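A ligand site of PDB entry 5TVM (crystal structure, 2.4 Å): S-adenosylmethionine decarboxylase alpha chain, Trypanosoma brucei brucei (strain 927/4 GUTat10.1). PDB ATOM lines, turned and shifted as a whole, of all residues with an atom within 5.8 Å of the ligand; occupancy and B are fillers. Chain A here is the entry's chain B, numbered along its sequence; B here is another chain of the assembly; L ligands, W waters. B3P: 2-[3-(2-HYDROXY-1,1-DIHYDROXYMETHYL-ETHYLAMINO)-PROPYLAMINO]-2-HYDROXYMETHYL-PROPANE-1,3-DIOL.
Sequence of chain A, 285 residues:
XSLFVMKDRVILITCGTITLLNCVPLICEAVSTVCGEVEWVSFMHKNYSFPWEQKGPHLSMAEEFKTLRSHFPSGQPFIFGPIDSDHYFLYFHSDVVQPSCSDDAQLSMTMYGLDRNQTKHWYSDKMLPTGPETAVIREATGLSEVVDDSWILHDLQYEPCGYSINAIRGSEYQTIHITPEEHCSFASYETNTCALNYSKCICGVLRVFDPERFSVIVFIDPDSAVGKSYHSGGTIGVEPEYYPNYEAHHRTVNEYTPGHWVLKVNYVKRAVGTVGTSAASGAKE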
ATOM      1  N   ASP A   8       6.204  17.407  -0.389  1.00  0.00           N
ATOM      2  CA  ASP A   8       5.396  16.221  -0.632  1.00  0.00           C
ATOM      3  C   ASP A   8       6.078  15.152  -1.482  1.00  0.00           C
ATOM      4  O   ASP A   8       5.450  14.126  -1.753  1.00  0.00           O
ATOM      5  CB  ASP A   8       4.087  16.616  -1.317  1.00  0.00           C
ATOM      6  CG  ASP A   8       4.300  17.090  -2.747  1.00  0.00           C
ATOM      7  OD1 ASP A   8       5.432  17.489  -3.077  1.00  0.00           O
ATOM      8  OD2 ASP A   8       3.338  17.054  -3.534  1.00  0.00           O
ATOM      9  N   ARG A   9       7.320  15.351  -1.915  1.00  0.00           N
ATOM     10  CA  ARG A   9       7.919  14.400  -2.839  1.00  0.00           C
ATOM     11  C   ARG A   9       9.434  14.465  -2.737  1.00  0.00           C
ATOM     12  O   ARG A   9      10.011  15.359  -2.125  1.00  0.00           O
ATOM     13  CB  ARG A   9       7.456  14.660  -4.274  1.00  0.00           C
ATOM     14  CG  ARG A   9       7.975  15.973  -4.868  1.00  0.00           C
ATOM     15  CD  ARG A   9       7.328  16.248  -6.225  1.00  0.00           C
ATOM     16  NE  ARG A   9       5.885  16.366  -6.122  1.00  0.00           N
ATOM     17  CZ  ARG A   9       5.057  16.374  -7.155  1.00  0.00           C
ATOM     18  NH1 ARG A   9       3.746  16.485  -6.956  1.00  0.00           N
ATOM     19  NH2 ARG A   9       5.519  16.259  -8.390  1.00  0.00           N
ATOM     20  N   GLU A  39       2.166   7.210  -2.170  1.00  0.00           N
ATOM     21  CA  GLU A  39       1.043   6.967  -3.058  1.00  0.00           C
ATOM     22  C   GLU A  39       1.404   6.996  -4.539  1.00  0.00           C
ATOM     23  O   GLU A  39       0.555   6.661  -5.361  1.00  0.00           O
ATOM     24  CB  GLU A  39      -0.068   8.004  -2.823  1.00  0.00           C
ATOM     25  CG  GLU A  39       0.344   9.452  -3.090  1.00  0.00           C
ATOM     26  CD  GLU A  39      -0.843  10.376  -3.292  1.00  0.00           C
ATOM     27  OE1 GLU A  39      -1.901   9.899  -3.765  1.00  0.00           O
ATOM     28  OE2 GLU A  39      -0.720  11.575  -2.968  1.00  0.00           O
ATOM     29  N   TRP A  40       2.628   7.373  -4.906  1.00  0.00           N
ATOM     30  CA  TRP A  40       3.004   7.523  -6.302  1.00  0.00           C
ATOM     31  C   TRP A  40       4.514   7.376  -6.416  1.00  0.00           C
ATOM     32  O   TRP A  40       5.251   8.154  -5.796  1.00  0.00           O
ATOM     33  CB  TRP A  40       2.542   8.872  -6.838  1.00  0.00           C
ATOM     34  CG  TRP A  40       2.873   9.139  -8.283  1.00  0.00           C
ATOM     35  CD1 TRP A  40       4.103   9.381  -8.819  1.00  0.00           C
ATOM     36  CD2 TRP A  40       1.945   9.201  -9.366  1.00  0.00           C
ATOM     37  NE1 TRP A  40       4.001   9.585 -10.173  1.00  0.00           N
ATOM     38  CE2 TRP A  40       2.686   9.487 -10.538  1.00  0.00           C
ATOM     39  CE3 TRP A  40       0.559   9.047  -9.471  1.00  0.00           C
ATOM     40  CZ2 TRP A  40       2.090   9.611 -11.784  1.00  0.00           C
ATOM     41  CZ3 TRP A  40      -0.037   9.171 -10.718  1.00  0.00           C
ATOM     42  CH2 TRP A  40       0.730   9.454 -11.862  1.00  0.00           C
ATOM     43  N   VAL A  96      -3.507   5.423  -5.174  1.00  0.00           N
ATOM     44  CA  VAL A  96      -4.281   6.641  -4.968  1.00  0.00           C
ATOM     45  C   VAL A  96      -5.658   6.212  -4.452  1.00  0.00           C
ATOM     46  O   VAL A  96      -6.552   5.865  -5.234  1.00  0.00           O
ATOM     47  CB  VAL A  96      -4.396   7.463  -6.257  1.00  0.00           C
ATOM     48  CG1 VAL A  96      -5.093   8.790  -5.978  1.00  0.00           C
ATOM     49  CG2 VAL A  96      -3.020   7.697  -6.858  1.00  0.00           C
ATOM     50  N   SER A 100      -7.549  12.951  -6.070  1.00  0.00           N
ATOM     51  CA  SER A 100      -6.987  14.259  -5.774  1.00  0.00           C
ATOM     52  C   SER A 100      -7.019  15.136  -7.024  1.00  0.00           C
ATOM     53  O   SER A 100      -7.693  14.823  -8.019  1.00  0.00           O
ATOM     54  CB  SER A 100      -5.555  14.095  -5.240  1.00  0.00           C
ATOM     55  OG  SER A 100      -5.515  13.204  -4.145  1.00  0.00           O
ATOM     56  N   CYS A 101      -6.306  16.254  -6.970  1.00  0.00           N
ATOM     57  CA  CYS A 101      -6.176  17.188  -8.080  1.00  0.00           C
ATOM     58  C   CYS A 101      -4.725  17.226  -8.509  1.00  0.00           C
ATOM     59  O   CYS A 101      -3.854  17.627  -7.724  1.00  0.00           O
ATOM     60  CB  CYS A 101      -6.670  18.577  -7.679  1.00  0.00           C
ATOM     61  SG  CYS A 101      -6.340  19.867  -8.904  1.00  0.00           S
ATOM     62  N   SER A 102      -4.460  16.824  -9.754  1.00  0.00           N
ATOM     63  CA  SER A 102      -3.098  16.737 -10.288  1.00  0.00           C
ATOM     64  C   SER A 102      -2.892  17.872 -11.267  1.00  0.00           C
ATOM     65  O   SER A 102      -3.464  17.874 -12.366  1.00  0.00           O
ATOM     66  CB  SER A 102      -2.866  15.379 -10.954  1.00  0.00           C
ATOM     67  OG  SER A 102      -3.045  14.317 -10.033  1.00  0.00           O
ATOM     68  N   ASP A 103      -2.057  18.846 -10.885  1.00  0.00           N
ATOM     69  CA  ASP A 103      -1.759  19.999 -11.731  1.00  0.00           C
ATOM     70  C   ASP A 103      -0.248  20.201 -11.867  1.00  0.00           C
ATOM     71  O   ASP A 103       0.209  21.320 -12.110  1.00  0.00           O
ATOM     72  CB  ASP A 103      -2.413  21.261 -11.177  1.00  0.00           C
ATOM     73  CG  ASP A 103      -1.986  21.580  -9.756  1.00  0.00           C
ATOM     74  OD1 ASP A 103      -1.657  20.632  -9.009  1.00  0.00           O
ATOM     75  OD2 ASP A 103      -1.989  22.768  -9.385  1.00  0.00           O
ATOM     76  N   ASP A 104       0.528  19.131 -11.716  1.00  0.00           N
ATOM     77  CA  ASP A 104       1.977  19.212 -11.864  1.00  0.00           C
ATOM     78  C   ASP A 104       2.362  19.236 -13.342  1.00  0.00           C
ATOM     79  O   ASP A 104       1.525  19.125 -14.243  1.00  0.00           O
ATOM     80  CB  ASP A 104       2.662  18.053 -11.143  1.00  0.00           C
ATOM     81  CG  ASP A 104       2.327  18.008  -9.667  1.00  0.00           C
ATOM     82  OD1 ASP A 104       2.027  19.073  -9.083  1.00  0.00           O
ATOM     83  OD2 ASP A 104       2.384  16.897  -9.087  1.00  0.00           O
ATOM     84  N   ALA A 105       3.666  19.362 -13.595  1.00  0.00           N
ATOM     85  CA  ALA A 105       4.197  19.342 -14.944  1.00  0.00           C
ATOM     86  C   ALA A 105       5.631  18.835 -14.891  1.00  0.00           C
ATOM     87  O   ALA A 105       6.356  19.090 -13.933  1.00  0.00           O
ATOM     88  CB  ALA A 105       4.145  20.729 -15.593  1.00  0.00           C
ATOM     89  N   GLN A 106       6.024  18.109 -15.937  1.00  0.00           N
ATOM     90  CA  GLN A 106       7.374  17.555 -16.025  1.00  0.00           C
ATOM     91  C   GLN A 106       7.816  17.590 -17.473  1.00  0.00           C
ATOM     92  O   GLN A 106       7.127  17.048 -18.343  1.00  0.00           O
ATOM     93  CB  GLN A 106       7.411  16.119 -15.475  1.00  0.00           C
ATOM     94  CG  GLN A 106       8.766  15.440 -15.583  1.00  0.00           C
ATOM     95  CD  GLN A 106       8.740  14.014 -15.071  1.00  0.00           C
ATOM     96  OE1 GLN A 106       7.801  13.609 -14.395  1.00  0.00           O
ATOM     97  NE2 GLN A 106       9.773  13.247 -15.408  1.00  0.00           N
ATOM     98  N   PHE A 219       5.169  14.926 -19.457  1.00  0.00           N
ATOM     99  CA  PHE A 219       4.123  14.313 -18.644  1.00  0.00           C
ATOM    100  C   PHE A 219       3.036  15.350 -18.389  1.00  0.00           C
ATOM    101  O   PHE A 219       3.292  16.403 -17.805  1.00  0.00           O
ATOM    102  CB  PHE A 219       4.689  13.797 -17.322  1.00  0.00           C
ATOM    103  CG  PHE A 219       5.469  12.523 -17.468  1.00  0.00           C
ATOM    104  CD1 PHE A 219       6.774  12.553 -17.914  1.00  0.00           C
ATOM    105  CD2 PHE A 219       4.898  11.306 -17.150  1.00  0.00           C
ATOM    106  CE1 PHE A 219       7.497  11.377 -18.046  1.00  0.00           C
ATOM    107  CE2 PHE A 219       5.605  10.131 -17.289  1.00  0.00           C
ATOM    108  CZ  PHE A 219       6.915  10.169 -17.731  1.00  0.00           C
ATOM    109  N   ILE A 220       1.809  15.036 -18.815  1.00  0.00           N
ATOM    110  CA  ILE A 220       0.693  15.969 -18.776  1.00  0.00           C
ATOM    111  C   ILE A 220      -0.279  15.487 -17.706  1.00  0.00           C
ATOM    112  O   ILE A 220      -0.838  14.389 -17.811  1.00  0.00           O
ATOM    113  CB  ILE A 220      -0.003  16.085 -20.135  1.00  0.00           C
ATOM    114  CG1 ILE A 220       0.933  16.782 -21.134  1.00  0.00           C
ATOM    115  CG2 ILE A 220      -1.336  16.819 -20.011  1.00  0.00           C
ATOM    116  CD1 ILE A 220       0.389  16.868 -22.550  1.00  0.00           C
ATOM    117  N   ASP A 221      -0.504  16.315 -16.686  1.00  0.00           N
ATOM    118  CA  ASP A 221      -1.524  16.033 -15.696  1.00  0.00           C
ATOM    119  C   ASP A 221      -2.865  16.617 -16.146  1.00  0.00           C
ATOM    120  O   ASP A 221      -2.902  17.596 -16.897  1.00  0.00           O
ATOM    121  CB  ASP A 221      -1.139  16.608 -14.345  1.00  0.00           C
ATOM    122  CG  ASP A 221       0.035  15.878 -13.717  1.00  0.00           C
ATOM    123  OD1 ASP A 221       0.311  14.733 -14.117  1.00  0.00           O
ATOM    124  OD2 ASP A 221       0.683  16.464 -12.822  1.00  0.00           O
ATOM    125  N   TYR A 256      -0.847   6.323 -19.487  1.00  0.00           N
ATOM    126  CA  TYR A 256      -0.322   5.223 -18.679  1.00  0.00           C
ATOM    127  C   TYR A 256      -1.186   4.938 -17.464  1.00  0.00           C
ATOM    128  O   TYR A 256      -1.317   3.774 -17.052  1.00  0.00           O
ATOM    129  CB  TYR A 256       1.127   5.505 -18.267  1.00  0.00           C
ATOM    130  CG  TYR A 256       1.343   6.774 -17.465  1.00  0.00           C
ATOM    131  CD1 TYR A 256       1.462   8.007 -18.096  1.00  0.00           C
ATOM    132  CD2 TYR A 256       1.469   6.722 -16.082  1.00  0.00           C
ATOM    133  CE1 TYR A 256       1.670   9.158 -17.365  1.00  0.00           C
ATOM    134  CE2 TYR A 256       1.678   7.873 -15.352  1.00  0.00           C
ATOM    135  CZ  TYR A 256       1.772   9.086 -15.989  1.00  0.00           C
ATOM    136  OH  TYR A 256       1.978  10.243 -15.267  1.00  0.00           O
ATOM    137  N   HIS A 260      -3.937  10.710 -16.835  1.00  0.00           N
ATOM    138  CA  HIS A 260      -2.577  11.212 -16.940  1.00  0.00           C
ATOM    139  C   HIS A 260      -1.943  10.700 -18.224  1.00  0.00           C
ATOM    140  O   HIS A 260      -1.984   9.501 -18.506  1.00  0.00           O
ATOM    141  CB  HIS A 260      -1.742  10.790 -15.722  1.00  0.00           C
ATOM    142  CG  HIS A 260      -2.302  11.257 -14.423  1.00  0.00           C
ATOM    143  ND1 HIS A 260      -3.473  10.756 -13.895  1.00  0.00           N
ATOM    144  CD2 HIS A 260      -1.856  12.181 -13.532  1.00  0.00           C
ATOM    145  CE1 HIS A 260      -3.719  11.354 -12.737  1.00  0.00           C
ATOM    146  NE2 HIS A 260      -2.753  12.224 -12.501  1.00  0.00           N
ATOM    147  N   TRP A 261      -1.342  11.612 -18.981  1.00  0.00           N
ATOM    148  CA  TRP A 261      -0.784  11.306 -20.286  1.00  0.00           C
ATOM    149  C   TRP A 261       0.693  11.645 -20.328  1.00  0.00           C
ATOM    150  O   TRP A 261       1.199  12.445 -19.542  1.00  0.00           O
ATOM    151  CB  TRP A 261      -1.533  12.069 -21.384  1.00  0.00           C
ATOM    152  CG  TRP A 261      -2.968  11.679 -21.493  1.00  0.00           C
ATOM    153  CD1 TRP A 261      -3.961  11.991 -20.619  1.00  0.00           C
ATOM    154  CD2 TRP A 261      -3.564  10.882 -22.521  1.00  0.00           C
ATOM    155  NE1 TRP A 261      -5.152  11.446 -21.054  1.00  0.00           N
ATOM    156  CE2 TRP A 261      -4.933  10.763 -22.211  1.00  0.00           C
ATOM    157  CE3 TRP A 261      -3.070  10.267 -23.678  1.00  0.00           C
ATOM    158  CZ2 TRP A 261      -5.820  10.056 -23.014  1.00  0.00           C
ATOM    159  CZ3 TRP A 261      -3.951   9.568 -24.479  1.00  0.00           C
ATOM    160  CH2 TRP A 261      -5.316   9.462 -24.149  1.00  0.00           C
ATOM    161  N   ARG B  34      15.963   8.350 -13.090  1.00  0.00           N
ATOM    162  CA  ARG B  34      15.113   9.283 -12.369  1.00  0.00           C
ATOM    163  C   ARG B  34      14.190   8.498 -11.453  1.00  0.00           C
ATOM    164  O   ARG B  34      13.455   7.622 -11.918  1.00  0.00           O
ATOM    165  CB  ARG B  34      14.304  10.159 -13.333  1.00  0.00           C
ATOM    166  CG  ARG B  34      13.503  11.243 -12.650  1.00  0.00           C
ATOM    167  CD  ARG B  34      12.688  12.056 -13.640  1.00  0.00           C
ATOM    168  NE  ARG B  34      12.107  13.233 -13.013  1.00  0.00           N
ATOM    169  CZ  ARG B  34      10.948  13.256 -12.364  1.00  0.00           C
ATOM    170  NH1 ARG B  34      10.220  12.151 -12.251  1.00  0.00           N
ATOM    171  NH2 ARG B  34      10.508  14.388 -11.824  1.00  0.00           N
ATOM    172  N   GLU B  36      11.199   9.145  -8.493  1.00  0.00           N
ATOM    173  CA  GLU B  36      10.304  10.128  -7.898  1.00  0.00           C
ATOM    174  C   GLU B  36       9.327   9.429  -6.975  1.00  0.00           C
ATOM    175  O   GLU B  36       8.714   8.428  -7.355  1.00  0.00           O
ATOM    176  CB  GLU B  36       9.542  10.917  -8.976  1.00  0.00           C
ATOM    177  CG  GLU B  36       8.673  12.033  -8.401  1.00  0.00           C
ATOM    178  CD  GLU B  36       8.060  12.921  -9.466  1.00  0.00           C
ATOM    179  OE1 GLU B  36       8.207  12.607 -10.663  1.00  0.00           O
ATOM    180  OE2 GLU B  36       7.442  13.942  -9.096  1.00  0.00           O
ATOM    181  N   ILE B  38       6.106  10.439  -4.345  1.00  0.00           N
ATOM    182  CA  ILE B  38       5.164  11.418  -3.813  1.00  0.00           C
ATOM    183  C   ILE B  38       4.382  10.752  -2.689  1.00  0.00           C
ATOM    184  O   ILE B  38       3.957   9.590  -2.830  1.00  0.00           O
ATOM    185  CB  ILE B  38       4.221  11.963  -4.904  1.00  0.00           C
ATOM    186  CG1 ILE B  38       5.016  12.462  -6.112  1.00  0.00           C
ATOM    187  CG2 ILE B  38       3.347  13.071  -4.332  1.00  0.00           C
ATOM    188  CD1 ILE B  38       4.160  12.782  -7.329  1.00  0.00           C
HETATM  189  C1  B3P L   1       1.022  12.837 -10.670  1.00  0.00           C
HETATM  190  C2  B3P L   1       0.800  13.518  -9.357  1.00  0.00           C
HETATM  191  C3  B3P L   1       2.476  12.938 -11.012  1.00  0.00           C
HETATM  192  N1  B3P L   1       2.752  14.265 -11.635  1.00  0.00           N
HETATM  193  C4  B3P L   1       4.067  14.215 -12.291  1.00  0.00           C
HETATM  194  C5  B3P L   1       4.461  15.577 -12.884  1.00  0.00           C
HETATM  195  C6  B3P L   1       5.165  13.725 -11.300  1.00  0.00           C
HETATM  196  C7  B3P L   1       3.983  13.166 -13.494  1.00  0.00           C
HETATM  197  N2  B3P L   1      -0.645  13.485  -9.035  1.00  0.00           N
HETATM  198  C8  B3P L   1      -0.824  13.170  -7.609  1.00  0.00           C
HETATM  199  C9  B3P L   1      -2.305  13.098  -7.230  1.00  0.00           C
HETATM  200  C10 B3P L   1      -0.068  14.203  -6.689  1.00  0.00           C
HETATM  201  C11 B3P L   1      -0.203  11.723  -7.331  1.00  0.00           C
HETATM  202  O1  B3P L   1      -2.880  12.151  -8.043  1.00  0.00           O
HETATM  203  O2  B3P L   1      -0.486  15.467  -7.048  1.00  0.00           O
HETATM  204  O3  B3P L   1      -0.445  11.399  -6.015  1.00  0.00           O
HETATM  205  O4  B3P L   1       3.384  16.050 -13.613  1.00  0.00           O
HETATM  206  O5  B3P L   1       5.141  14.583 -10.226  1.00  0.00           O
HETATM  207  O6  B3P L   1       2.806  13.388 -14.174  1.00  0.00           O
HETATM  208  O   HOH W   1       6.231  10.560 -11.484  1.00  0.00           O
HETATM  209  O   HOH W   2       1.125  12.573 -16.442  1.00  0.00           O
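Trp 40 touches the ligand (CZ2 to C3, 3.4 Å). CB of Ser 100 touches C9 of the ligand, 3.9 Å away. Gln 106 touches the ligand. CB of Phe 219 touches O6 of the ligand, at 3.7 Å. Ile 38 of chain B touches the ligand. Hydrophobic or aromatic side chains within 4 Å of the ligand: Trp 40, Phe 219 and Ile 38 of chain B. Within 4 Å of the ligand: Arg 9, Glu 39, Trp 40, Ser 100, Ser 102, Asp 104, Ala 105, Gln 106, Phe 219, Asp 221, Tyr 256, Glu 36 of chain B and Ile 38 of chain B.
The side-chain hydroxyl (OH) of Tyr 256 sits at hydrogen-bond distance from an oxygen (O6) of the ligand, 3.4 Å away. N1 of the ligand is in salt-bridge range of OD2 of Asp 221 (3.2 Å). The side-chain hydroxyl (OG) of Ser 102 is in hydrogen-bond range of a nitrogen (N2) of the ligand, at 2.7 Å. The side-chain carboxylate (OE2) of Glu 39 lies close to an oxygen (O3) of the ligand (3.1 Å). A nitrogen (N1) of the ligand lies within salt-bridge range of the side-chain carboxylate (OD2) of Asp 104 (3.7 Å). An oxygen (O4) of the ligand lies within hydrogen-bond range of the backbone NH (N) of Ala 105. The guanidinium group (NH2) of Arg 9 sits at hydrogen-bond distance from an oxygen (O5) of the ligand. The side-chain carboxylate (OE2) of Glu 36 of chain B sits at hydrogen-bond distance from an oxygen (O5) of the ligand (2.6 Å).
The backbone NH (N) of Asp 104 is in hydrogen-bond range of the side-chain carboxylate (OD2) of Asp 221 (2.9 Å). The side-chain hydroxyl (OG) of Ser 102 lies within hydrogen-bond range of a ring nitrogen (NE2) of His 260 (3.2 Å). N of Glu 39 sits at hydrogen-bond distance from O of Ile 38 of chain B. The side-chain amide nitrogen (NE2) of Gln 106 lies close to the guanidinium group (NE) of Arg 34 of chain B, 3.3 Å away. The backbone carbonyl oxygen (O) of Trp 40 lies within hydrogen-bond range of the backbone NH (N) of Ile 38 of chain B. NH1 of Arg 34 of chain B is in salt-bridge range of OE1 of Glu 36 of chain B (2.6 Å). The side-chain carboxylate of Asp 104 is in salt-bridge range of the guanidinium group of Arg 9, 2.6 Å away. The guanidinium group (NE) of Arg 9 is in salt-bridge range of the side-chain carboxylate (OD1) of Asp 8, at 3.3 Å.
Water W1 bridges the indole nitrogen of Trp 40 (2.8 Å) and the side-chain carboxylate of Glu 36 of chain B (3.0 Å).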
